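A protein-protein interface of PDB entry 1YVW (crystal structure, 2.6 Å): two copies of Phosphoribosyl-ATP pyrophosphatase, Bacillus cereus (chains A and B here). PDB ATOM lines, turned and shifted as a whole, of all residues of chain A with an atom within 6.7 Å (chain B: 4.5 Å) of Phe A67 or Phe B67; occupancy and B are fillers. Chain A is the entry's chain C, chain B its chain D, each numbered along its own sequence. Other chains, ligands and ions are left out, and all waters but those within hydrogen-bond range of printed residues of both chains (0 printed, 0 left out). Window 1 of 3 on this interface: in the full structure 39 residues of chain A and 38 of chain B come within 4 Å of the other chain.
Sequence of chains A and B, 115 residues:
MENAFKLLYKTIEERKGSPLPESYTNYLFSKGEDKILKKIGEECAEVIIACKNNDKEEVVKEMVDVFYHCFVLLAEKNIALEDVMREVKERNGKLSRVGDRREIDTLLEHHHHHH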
ATOM      1  N   PHE A   5      13.380  13.524   1.224  1.00  0.00           N
ATOM      2  CA  PHE A   5      12.973  12.330   0.479  1.00  0.00           C
ATOM      3  C   PHE A   5      14.174  11.820  -0.310  1.00  0.00           C
ATOM      4  O   PHE A   5      14.380  10.612  -0.430  1.00  0.00           O
ATOM      5  CB  PHE A   5      11.820  12.645  -0.477  1.00  0.00           C
ATOM      6  CG  PHE A   5      10.479  12.668   0.179  1.00  0.00           C
ATOM      7  CD1 PHE A   5       9.906  11.496   0.664  1.00  0.00           C
ATOM      8  CD2 PHE A   5       9.775  13.852   0.304  1.00  0.00           C
ATOM      9  CE1 PHE A   5       8.637  11.510   1.262  1.00  0.00           C
ATOM     10  CE2 PHE A   5       8.509  13.878   0.900  1.00  0.00           C
ATOM     11  CZ  PHE A   5       7.944  12.706   1.378  1.00  0.00           C
ATOM     12  N   LEU A   8      16.628  10.156   2.101  1.00  0.00           N
ATOM     13  CA  LEU A   8      16.143   8.827   2.448  1.00  0.00           C
ATOM     14  C   LEU A   8      16.501   7.840   1.347  1.00  0.00           C
ATOM     15  O   LEU A   8      17.022   6.751   1.617  1.00  0.00           O
ATOM     16  CB  LEU A   8      14.622   8.862   2.653  1.00  0.00           C
ATOM     17  CG  LEU A   8      13.909   7.581   3.101  1.00  0.00           C
ATOM     18  CD1 LEU A   8      14.491   7.074   4.424  1.00  0.00           C
ATOM     19  CD2 LEU A   8      12.416   7.844   3.243  1.00  0.00           C
ATOM     20  N   ILE A  12      19.166   4.596   1.374  1.00  0.00           N
ATOM     21  CA  ILE A  12      18.697   3.263   1.005  1.00  0.00           C
ATOM     22  C   ILE A  12      19.598   2.701  -0.098  1.00  0.00           C
ATOM     23  O   ILE A  12      19.903   1.509  -0.107  1.00  0.00           O
ATOM     24  CB  ILE A  12      17.200   3.317   0.562  1.00  0.00           C
ATOM     25  CG1 ILE A  12      16.305   3.548   1.781  1.00  0.00           C
ATOM     26  CG2 ILE A  12      16.788   2.045  -0.175  1.00  0.00           C
ATOM     27  CD1 ILE A  12      14.877   3.884   1.462  1.00  0.00           C
ATOM     28  N   GLU A  43       1.361  -2.061   4.945  1.00  0.00           N
ATOM     29  CA  GLU A  43       1.478  -0.677   5.387  1.00  0.00           C
ATOM     30  C   GLU A  43       0.346   0.195   4.876  1.00  0.00           C
ATOM     31  O   GLU A  43      -0.105   1.104   5.568  1.00  0.00           O
ATOM     32  CB  GLU A  43       2.814  -0.087   4.940  1.00  0.00           C
ATOM     33  CG  GLU A  43       3.756   0.244   6.061  1.00  0.00           C
ATOM     34  CD  GLU A  43       4.147  -0.957   6.879  1.00  0.00           C
ATOM     35  OE1 GLU A  43       5.061  -1.686   6.447  1.00  0.00           O
ATOM     36  OE2 GLU A  43       3.553  -1.163   7.959  1.00  0.00           O
ATOM     37  N   GLU A  62       2.812   5.461   9.503  1.00  0.00           N
ATOM     38  CA  GLU A  62       2.503   4.471   8.491  1.00  0.00           C
ATOM     39  C   GLU A  62       2.685   4.988   7.063  1.00  0.00           C
ATOM     40  O   GLU A  62       3.144   4.237   6.187  1.00  0.00           O
ATOM     41  CB  GLU A  62       1.092   3.912   8.691  1.00  0.00           C
ATOM     42  CG  GLU A  62       0.928   3.084   9.959  1.00  0.00           C
ATOM     43  CD  GLU A  62       1.977   1.990  10.127  1.00  0.00           C
ATOM     44  OE1 GLU A  62       2.505   1.453   9.121  1.00  0.00           O
ATOM     45  OE2 GLU A  62       2.264   1.652  11.290  1.00  0.00           O
ATOM     46  N   MET A  63       2.353   6.258   6.837  1.00  0.00           N
ATOM     47  CA  MET A  63       2.504   6.827   5.511  1.00  0.00           C
ATOM     48  C   MET A  63       3.985   6.861   5.153  1.00  0.00           C
ATOM     49  O   MET A  63       4.370   6.456   4.058  1.00  0.00           O
ATOM     50  CB  MET A  63       1.886   8.227   5.425  1.00  0.00           C
ATOM     51  CG  MET A  63       1.825   8.734   4.013  1.00  0.00           C
ATOM     52  SD  MET A  63       1.084  10.484   3.942  1.00  0.00           S
ATOM     53  CE  MET A  63      -0.717   9.985   4.384  1.00  0.00           C
ATOM     54  N   VAL A  64       4.812   7.290   6.101  1.00  0.00           N
ATOM     55  CA  VAL A  64       6.263   7.347   5.891  1.00  0.00           C
ATOM     56  C   VAL A  64       6.814   5.933   5.717  1.00  0.00           C
ATOM     57  O   VAL A  64       7.779   5.722   5.006  1.00  0.00           O
ATOM     58  CB  VAL A  64       6.996   8.101   7.048  1.00  0.00           C
ATOM     59  CG1 VAL A  64       8.529   7.977   6.908  1.00  0.00           C
ATOM     60  CG2 VAL A  64       6.605   9.575   7.024  1.00  0.00           C
ATOM     61  N   ASP A  65       6.161   4.969   6.354  1.00  0.00           N
ATOM     62  CA  ASP A  65       6.531   3.571   6.249  1.00  0.00           C
ATOM     63  C   ASP A  65       6.298   3.138   4.802  1.00  0.00           C
ATOM     64  O   ASP A  65       7.141   2.473   4.201  1.00  0.00           O
ATOM     65  CB  ASP A  65       5.655   2.733   7.164  1.00  0.00           C
ATOM     66  CG  ASP A  65       6.449   1.926   8.149  1.00  0.00           C
ATOM     67  OD1 ASP A  65       7.318   1.128   7.718  1.00  0.00           O
ATOM     68  OD2 ASP A  65       6.189   2.086   9.362  1.00  0.00           O
ATOM     69  N   VAL A  66       5.152   3.531   4.247  1.00  0.00           N
ATOM     70  CA  VAL A  66       4.807   3.211   2.869  1.00  0.00           C
ATOM     71  C   VAL A  66       5.852   3.824   1.943  1.00  0.00           C
ATOM     72  O   VAL A  66       6.366   3.152   1.056  1.00  0.00           O
ATOM     73  CB  VAL A  66       3.383   3.742   2.482  1.00  0.00           C
ATOM     74  CG1 VAL A  66       3.096   3.498   1.022  1.00  0.00           C
ATOM     75  CG2 VAL A  66       2.306   3.053   3.309  1.00  0.00           C
ATOM     76  N   PHE A  67       6.198   5.085   2.185  1.00  0.00           N
ATOM     77  CA  PHE A  67       7.186   5.785   1.371  1.00  0.00           C
ATOM     78  C   PHE A  67       8.570   5.138   1.435  1.00  0.00           C
ATOM     79  O   PHE A  67       9.253   5.003   0.410  1.00  0.00           O
ATOM     80  CB  PHE A  67       7.285   7.260   1.772  1.00  0.00           C
ATOM     81  CG  PHE A  67       6.023   8.044   1.526  1.00  0.00           C
ATOM     82  CD1 PHE A  67       4.946   7.482   0.842  1.00  0.00           C
ATOM     83  CD2 PHE A  67       5.907   9.342   1.985  1.00  0.00           C
ATOM     84  CE1 PHE A  67       3.777   8.206   0.616  1.00  0.00           C
ATOM     85  CE2 PHE A  67       4.748  10.079   1.766  1.00  0.00           C
ATOM     86  CZ  PHE A  67       3.679   9.507   1.082  1.00  0.00           C
ATOM     87  N   TYR A  68       8.975   4.751   2.640  1.00  0.00           N
ATOM     88  CA  TYR A  68      10.255   4.101   2.837  1.00  0.00           C
ATOM     89  C   TYR A  68      10.328   2.810   2.017  1.00  0.00           C
ATOM     90  O   TYR A  68      11.308   2.576   1.321  1.00  0.00           O
ATOM     91  CB  TYR A  68      10.480   3.814   4.331  1.00  0.00           C
ATOM     92  CG  TYR A  68      11.544   2.773   4.619  1.00  0.00           C
ATOM     93  CD1 TYR A  68      12.898   3.114   4.676  1.00  0.00           C
ATOM     94  CD2 TYR A  68      11.194   1.434   4.779  1.00  0.00           C
ATOM     95  CE1 TYR A  68      13.885   2.139   4.875  1.00  0.00           C
ATOM     96  CE2 TYR A  68      12.160   0.453   4.976  1.00  0.00           C
ATOM     97  CZ  TYR A  68      13.503   0.806   5.016  1.00  0.00           C
ATOM     98  OH  TYR A  68      14.451  -0.192   5.109  1.00  0.00           O
ATOM     99  N   HIS A  69       9.275   1.999   2.073  1.00  0.00           N
ATOM    100  CA  HIS A  69       9.264   0.745   1.344  1.00  0.00           C
ATOM    101  C   HIS A  69       9.181   0.943  -0.172  1.00  0.00           C
ATOM    102  O   HIS A  69       9.746   0.158  -0.937  1.00  0.00           O
ATOM    103  CB  HIS A  69       8.165  -0.171   1.874  1.00  0.00           C
ATOM    104  CG  HIS A  69       8.404  -0.647   3.270  1.00  0.00           C
ATOM    105  ND1 HIS A  69       9.103  -1.804   3.556  1.00  0.00           N
ATOM    106  CD2 HIS A  69       8.031  -0.145   4.467  1.00  0.00           C
ATOM    107  CE1 HIS A  69       9.145  -1.990   4.854  1.00  0.00           C
ATOM    108  NE2 HIS A  69       8.495  -0.991   5.437  1.00  0.00           N
ATOM    109  N   CYS A  70       8.503   2.002  -0.600  1.00  0.00           N
ATOM    110  CA  CYS A  70       8.416   2.321  -2.024  1.00  0.00           C
ATOM    111  C   CYS A  70       9.814   2.688  -2.545  1.00  0.00           C
ATOM    112  O   CYS A  70      10.187   2.304  -3.648  1.00  0.00           O
ATOM    113  CB  CYS A  70       7.444   3.478  -2.273  1.00  0.00           C
ATOM    114  SG  CYS A  70       5.699   3.010  -2.239  1.00  0.00           S
ATOM    115  N   PHE A  71      10.593   3.414  -1.737  1.00  0.00           N
ATOM    116  CA  PHE A  71      11.955   3.792  -2.130  1.00  0.00           C
ATOM    117  C   PHE A  71      12.863   2.575  -2.153  1.00  0.00           C
ATOM    118  O   PHE A  71      13.685   2.427  -3.056  1.00  0.00           O
ATOM    119  CB  PHE A  71      12.525   4.870  -1.218  1.00  0.00           C
ATOM    120  CG  PHE A  71      11.925   6.232  -1.453  1.00  0.00           C
ATOM    121  CD1 PHE A  71      12.481   7.361  -0.858  1.00  0.00           C
ATOM    122  CD2 PHE A  71      10.796   6.390  -2.264  1.00  0.00           C
ATOM    123  CE1 PHE A  71      11.921   8.621  -1.069  1.00  0.00           C
ATOM    124  CE2 PHE A  71      10.236   7.642  -2.475  1.00  0.00           C
ATOM    125  CZ  PHE A  71      10.799   8.760  -1.879  1.00  0.00           C
ATOM    126  N   VAL A  72      12.698   1.681  -1.178  1.00  0.00           N
ATOM    127  CA  VAL A  72      13.483   0.462  -1.145  1.00  0.00           C
ATOM    128  C   VAL A  72      13.167  -0.318  -2.425  1.00  0.00           C
ATOM    129  O   VAL A  72      14.072  -0.847  -3.070  1.00  0.00           O
ATOM    130  CB  VAL A  72      13.143  -0.398   0.103  1.00  0.00           C
ATOM    131  CG1 VAL A  72      13.816  -1.762   0.016  1.00  0.00           C
ATOM    132  CG2 VAL A  72      13.569   0.349   1.379  1.00  0.00           C
ATOM    133  N   LEU A  74      12.161   0.919  -5.299  1.00  0.00           N
ATOM    134  CA  LEU A  74      12.774   1.613  -6.430  1.00  0.00           C
ATOM    135  C   LEU A  74      14.228   1.151  -6.593  1.00  0.00           C
ATOM    136  O   LEU A  74      14.633   0.713  -7.676  1.00  0.00           O
ATOM    137  CB  LEU A  74      12.732   3.129  -6.231  1.00  0.00           C
ATOM    138  CG  LEU A  74      11.362   3.797  -6.337  1.00  0.00           C
ATOM    139  CD1 LEU A  74      11.502   5.289  -6.080  1.00  0.00           C
ATOM    140  CD2 LEU A  74      10.764   3.548  -7.721  1.00  0.00           C
ATOM    141  N   VAL A  84      10.962   9.382 -10.755  1.00  0.00           N
ATOM    142  CA  VAL A  84       9.796   9.593  -9.914  1.00  0.00           C
ATOM    143  C   VAL A  84       9.558  11.089  -9.784  1.00  0.00           C
ATOM    144  O   VAL A  84       8.435  11.568  -9.949  1.00  0.00           O
ATOM    145  CB  VAL A  84      10.007   8.970  -8.512  1.00  0.00           C
ATOM    146  CG1 VAL A  84       8.904   9.413  -7.555  1.00  0.00           C
ATOM    147  CG2 VAL A  84      10.054   7.441  -8.619  1.00  0.00           C
ATOM    148  N   VAL A  88       6.431  13.487 -10.655  1.00  0.00           N
ATOM    149  CA  VAL A  88       5.793  14.346  -9.657  1.00  0.00           C
ATOM    150  C   VAL A  88       5.649  15.761 -10.212  1.00  0.00           C
ATOM    151  O   VAL A  88       4.604  16.384 -10.057  1.00  0.00           O
ATOM    152  CB  VAL A  88       6.589  14.381  -8.327  1.00  0.00           C
ATOM    153  CG1 VAL A  88       5.922  15.337  -7.335  1.00  0.00           C
ATOM    154  CG2 VAL A  88       6.681  12.987  -7.730  1.00  0.00           C
ATOM    155  N   PHE B   5       7.736  17.642  -4.026  1.00  0.00           N
ATOM    156  CA  PHE B   5       6.725  17.025  -3.176  1.00  0.00           C
ATOM    157  C   PHE B   5       5.986  18.134  -2.424  1.00  0.00           C
ATOM    158  O   PHE B   5       4.771  18.067  -2.236  1.00  0.00           O
ATOM    159  CB  PHE B   5       7.368  16.056  -2.189  1.00  0.00           C
ATOM    160  CG  PHE B   5       7.716  14.726  -2.789  1.00  0.00           C
ATOM    161  CD1 PHE B   5       6.712  13.838  -3.155  1.00  0.00           C
ATOM    162  CD2 PHE B   5       9.041  14.350  -2.966  1.00  0.00           C
ATOM    163  CE1 PHE B   5       7.022  12.589  -3.688  1.00  0.00           C
ATOM    164  CE2 PHE B   5       9.365  13.099  -3.498  1.00  0.00           C
ATOM    165  CZ  PHE B   5       8.354  12.218  -3.858  1.00  0.00           C
ATOM    166  N   MET B  63       3.219   4.764  -8.422  1.00  0.00           N
ATOM    167  CA  MET B  63       3.805   5.163  -7.157  1.00  0.00           C
ATOM    168  C   MET B  63       3.485   6.637  -6.886  1.00  0.00           C
ATOM    169  O   MET B  63       3.053   6.981  -5.792  1.00  0.00           O
ATOM    170  CB  MET B  63       5.323   4.928  -7.137  1.00  0.00           C
ATOM    171  CG  MET B  63       5.921   5.181  -5.769  1.00  0.00           C
ATOM    172  SD  MET B  63       7.776   4.878  -5.767  1.00  0.00           S
ATOM    173  CE  MET B  63       7.674   2.942  -5.927  1.00  0.00           C
ATOM    174  N   VAL B  64       3.632   7.477  -7.909  1.00  0.00           N
ATOM    175  CA  VAL B  64       3.327   8.904  -7.775  1.00  0.00           C
ATOM    176  C   VAL B  64       1.825   9.086  -7.527  1.00  0.00           C
ATOM    177  O   VAL B  64       1.414  10.006  -6.827  1.00  0.00           O
ATOM    178  CB  VAL B  64       3.812   9.720  -9.015  1.00  0.00           C
ATOM    179  CG1 VAL B  64       3.273  11.173  -8.981  1.00  0.00           C
ATOM    180  CG2 VAL B  64       5.337   9.720  -9.052  1.00  0.00           C
ATOM    181  N   ASP B  65       1.027   8.171  -8.066  1.00  0.00           N
ATOM    182  CA  ASP B  65      -0.414   8.182  -7.880  1.00  0.00           C
ATOM    183  C   ASP B  65      -0.701   7.928  -6.396  1.00  0.00           C
ATOM    184  O   ASP B  65      -1.557   8.577  -5.788  1.00  0.00           O
ATOM    185  CB  ASP B  65      -1.044   7.077  -8.709  1.00  0.00           C
ATOM    186  CG  ASP B  65      -2.064   7.587  -9.696  1.00  0.00           C
ATOM    187  OD1 ASP B  65      -3.019   8.289  -9.279  1.00  0.00           O
ATOM    188  OD2 ASP B  65      -1.918   7.264 -10.892  1.00  0.00           O
ATOM    189  N   VAL B  66       0.033   6.984  -5.814  1.00  0.00           N
ATOM    190  CA  VAL B  66      -0.126   6.677  -4.404  1.00  0.00           C
ATOM    191  C   VAL B  66       0.255   7.914  -3.577  1.00  0.00           C
ATOM    192  O   VAL B  66      -0.480   8.306  -2.666  1.00  0.00           O
ATOM    193  CB  VAL B  66       0.755   5.467  -3.971  1.00  0.00           C
ATOM    194  CG1 VAL B  66       0.676   5.258  -2.451  1.00  0.00           C
ATOM    195  CG2 VAL B  66       0.317   4.200  -4.700  1.00  0.00           C
ATOM    196  N   PHE B  67       1.364   8.557  -3.940  1.00  0.00           N
ATOM    197  CA  PHE B  67       1.828   9.749  -3.234  1.00  0.00           C
ATOM    198  C   PHE B  67       0.845  10.911  -3.331  1.00  0.00           C
ATOM    199  O   PHE B  67       0.597  11.614  -2.344  1.00  0.00           O
ATOM    200  CB  PHE B  67       3.203  10.195  -3.742  1.00  0.00           C
ATOM    201  CG  PHE B  67       4.298   9.188  -3.489  1.00  0.00           C
ATOM    202  CD1 PHE B  67       4.054   8.034  -2.735  1.00  0.00           C
ATOM    203  CD2 PHE B  67       5.572   9.400  -3.993  1.00  0.00           C
ATOM    204  CE1 PHE B  67       5.055   7.111  -2.493  1.00  0.00           C
ATOM    205  CE2 PHE B  67       6.595   8.478  -3.757  1.00  0.00           C
ATOM    206  CZ  PHE B  67       6.339   7.328  -3.000  1.00  0.00           C
ATOM    207  N   TYR B  68       0.288  11.109  -4.522  1.00  0.00           N
ATOM    208  CA  TYR B  68      -0.665  12.166  -4.732  1.00  0.00           C
ATOM    209  C   TYR B  68      -1.885  11.985  -3.826  1.00  0.00           C
ATOM    210  O   TYR B  68      -2.316  12.925  -3.158  1.00  0.00           O
ATOM    211  CB  TYR B  68      -1.073  12.230  -6.205  1.00  0.00           C
ATOM    212  CG  TYR B  68      -2.362  12.960  -6.445  1.00  0.00           C
ATOM    213  CD1 TYR B  68      -2.395  14.354  -6.549  1.00  0.00           C
ATOM    214  CD2 TYR B  68      -3.568  12.256  -6.548  1.00  0.00           C
ATOM    215  CE1 TYR B  68      -3.612  15.038  -6.750  1.00  0.00           C
ATOM    216  CE2 TYR B  68      -4.781  12.920  -6.743  1.00  0.00           C
ATOM    217  CZ  TYR B  68      -4.798  14.310  -6.843  1.00  0.00           C
ATOM    218  OH  TYR B  68      -6.005  14.950  -7.027  1.00  0.00           O
ATOM    219  N   HIS B  69      -2.430  10.774  -3.798  1.00  0.00           N
ATOM    220  CA  HIS B  69      -3.587  10.484  -2.968  1.00  0.00           C
ATOM    221  C   HIS B  69      -3.274  10.555  -1.469  1.00  0.00           C
ATOM    222  O   HIS B  69      -4.139  10.906  -0.677  1.00  0.00           O
ATOM    223  CB  HIS B  69      -4.210   9.146  -3.353  1.00  0.00           C
ATOM    224  CG  HIS B  69      -4.832   9.149  -4.713  1.00  0.00           C
ATOM    225  ND1 HIS B  69      -6.152   9.546  -4.929  1.00  0.00           N
ATOM    226  CD2 HIS B  69      -4.348   8.815  -5.917  1.00  0.00           C
ATOM    227  CE1 HIS B  69      -6.427   9.444  -6.204  1.00  0.00           C
ATOM    228  NE2 HIS B  69      -5.355   9.004  -6.845  1.00  0.00           N
ATOM    229  N   CYS B  70      -2.040  10.235  -1.081  1.00  0.00           N
ATOM    230  CA  CYS B  70      -1.649  10.337   0.317  1.00  0.00           C
ATOM    231  C   CYS B  70      -1.620  11.835   0.719  1.00  0.00           C
ATOM    232  O   CYS B  70      -2.052  12.205   1.814  1.00  0.00           O
ATOM    233  CB  CYS B  70      -0.277   9.679   0.569  1.00  0.00           C
ATOM    234  SG  CYS B  70      -0.297   7.840   0.672  1.00  0.00           S
ATOM    235  N   PHE B  71      -1.142  12.685  -0.180  1.00  0.00           N
ATOM    236  CA  PHE B  71      -1.101  14.120   0.095  1.00  0.00           C
ATOM    237  C   PHE B  71      -2.514  14.714   0.135  1.00  0.00           C
ATOM    238  O   PHE B  71      -2.810  15.567   0.971  1.00  0.00           O
ATOM    239  CB  PHE B  71      -0.238  14.861  -0.924  1.00  0.00           C
ATOM    240  CG  PHE B  71       1.237  14.646  -0.730  1.00  0.00           C
ATOM    241  CD1 PHE B  71       2.157  15.413  -1.432  1.00  0.00           C
ATOM    242  CD2 PHE B  71       1.709  13.666   0.141  1.00  0.00           C
ATOM    243  CE1 PHE B  71       3.513  15.214  -1.277  1.00  0.00           C
ATOM    244  CE2 PHE B  71       3.068  13.457   0.309  1.00  0.00           C
ATOM    245  CZ  PHE B  71       3.980  14.234  -0.405  1.00  0.00           C
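The backbone carbonyl oxygen of Val A66 sits at hydrogen-bond distance from the side-chain sulfur of Cys A70 (3.4 Å).
SG of Cys B70 is in hydrogen-bond range of O of Val B66.
Phe A5 touches Phe B5.
O of Cys B70 touches CE of Met A63 (3.6 Å).
Phe B67 touches Phe A67 (CE1 to CD1, 3.4 Å).
Cys B70 touches Phe A67 (CB to CZ, 3.99 Å).
Cys A70 touches Met B63 (O to CE, 3.5 Å).
Phe A71 touches Phe B67 (CE2 to CZ, 3.9 Å).
CD2 of Leu A74 touches CE of Met B63, 3.6 Å away.
O of Val A84 touches CG2 of Val B64, at 3.7 Å.
CG2 of Val A88 touches CG2 of Val B64, at 3.8 Å.
Of the printed residues of chain B, Phe A5 touches Phe B5.
Of the printed residues of chain B, Phe A67 touches Phe B67 (3.4 Å) and Cys B70 (3.99 Å).
Of the printed residues of chain B, Cys A70 touches Met B63.
Of the printed residues of chain B, Val A88 touches Val B64 (3.8 Å).
Of the printed residues of chain A, Met B63 touches Cys A70 (3.5 Å) and Leu A74 (3.6 Å).
Of the printed residues of chain A, Val B64 touches Val A84 and Val A88.
Of chain A, only Phe A67 (3.4 Å) and Phe A71 (3.9 Å) come within 4 Å of Phe B67.
The nearest residue of chain A that does not touch Phe B67 is Cys A70 (4.1 Å).
The nearest printed residue of chain A that does not touch Cys B70 is Val A66 (5.5 Å).
Of the 10 printed residues of chain B, 5 touch a printed residue of chain A.
Printed residues of chain B that touch a printed residue of chain A: Phe B5, Met B63, Val B64, Phe B67 and Cys B70.
Hydrophobic or aromatic side chains of chain B within 4 Å of the printed part of chain A: Phe B5, Met B63, Val B64 and Phe B67.
Of the 18 printed residues of chain A, 8 touch a printed residue of chain B.
Hydrophobic or aromatic side chains of chain A that line the printed part of chain B: Phe A5, Met A63, Phe A67, Phe A71, Leu A74, Val A84 and Val A88.
Among the printed residues, no Asp or Glu carboxylate lies within 4 Å of a Lys or Arg side-chain nitrogen of the other chain.
Phe B5 touches its own counterpart, Phe A5.
Met A63 touches Cys B70, and with the chains exchanged Cys A70 touches Met B63.
Phe A67 touches Cys B70, but with the chains exchanged Cys A70 does not touch Phe B67 (4.1 Å).
Phe A71 touches Phe B67, but with the chains exchanged Phe A67 does not touch Phe B71 (4.04 Å).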
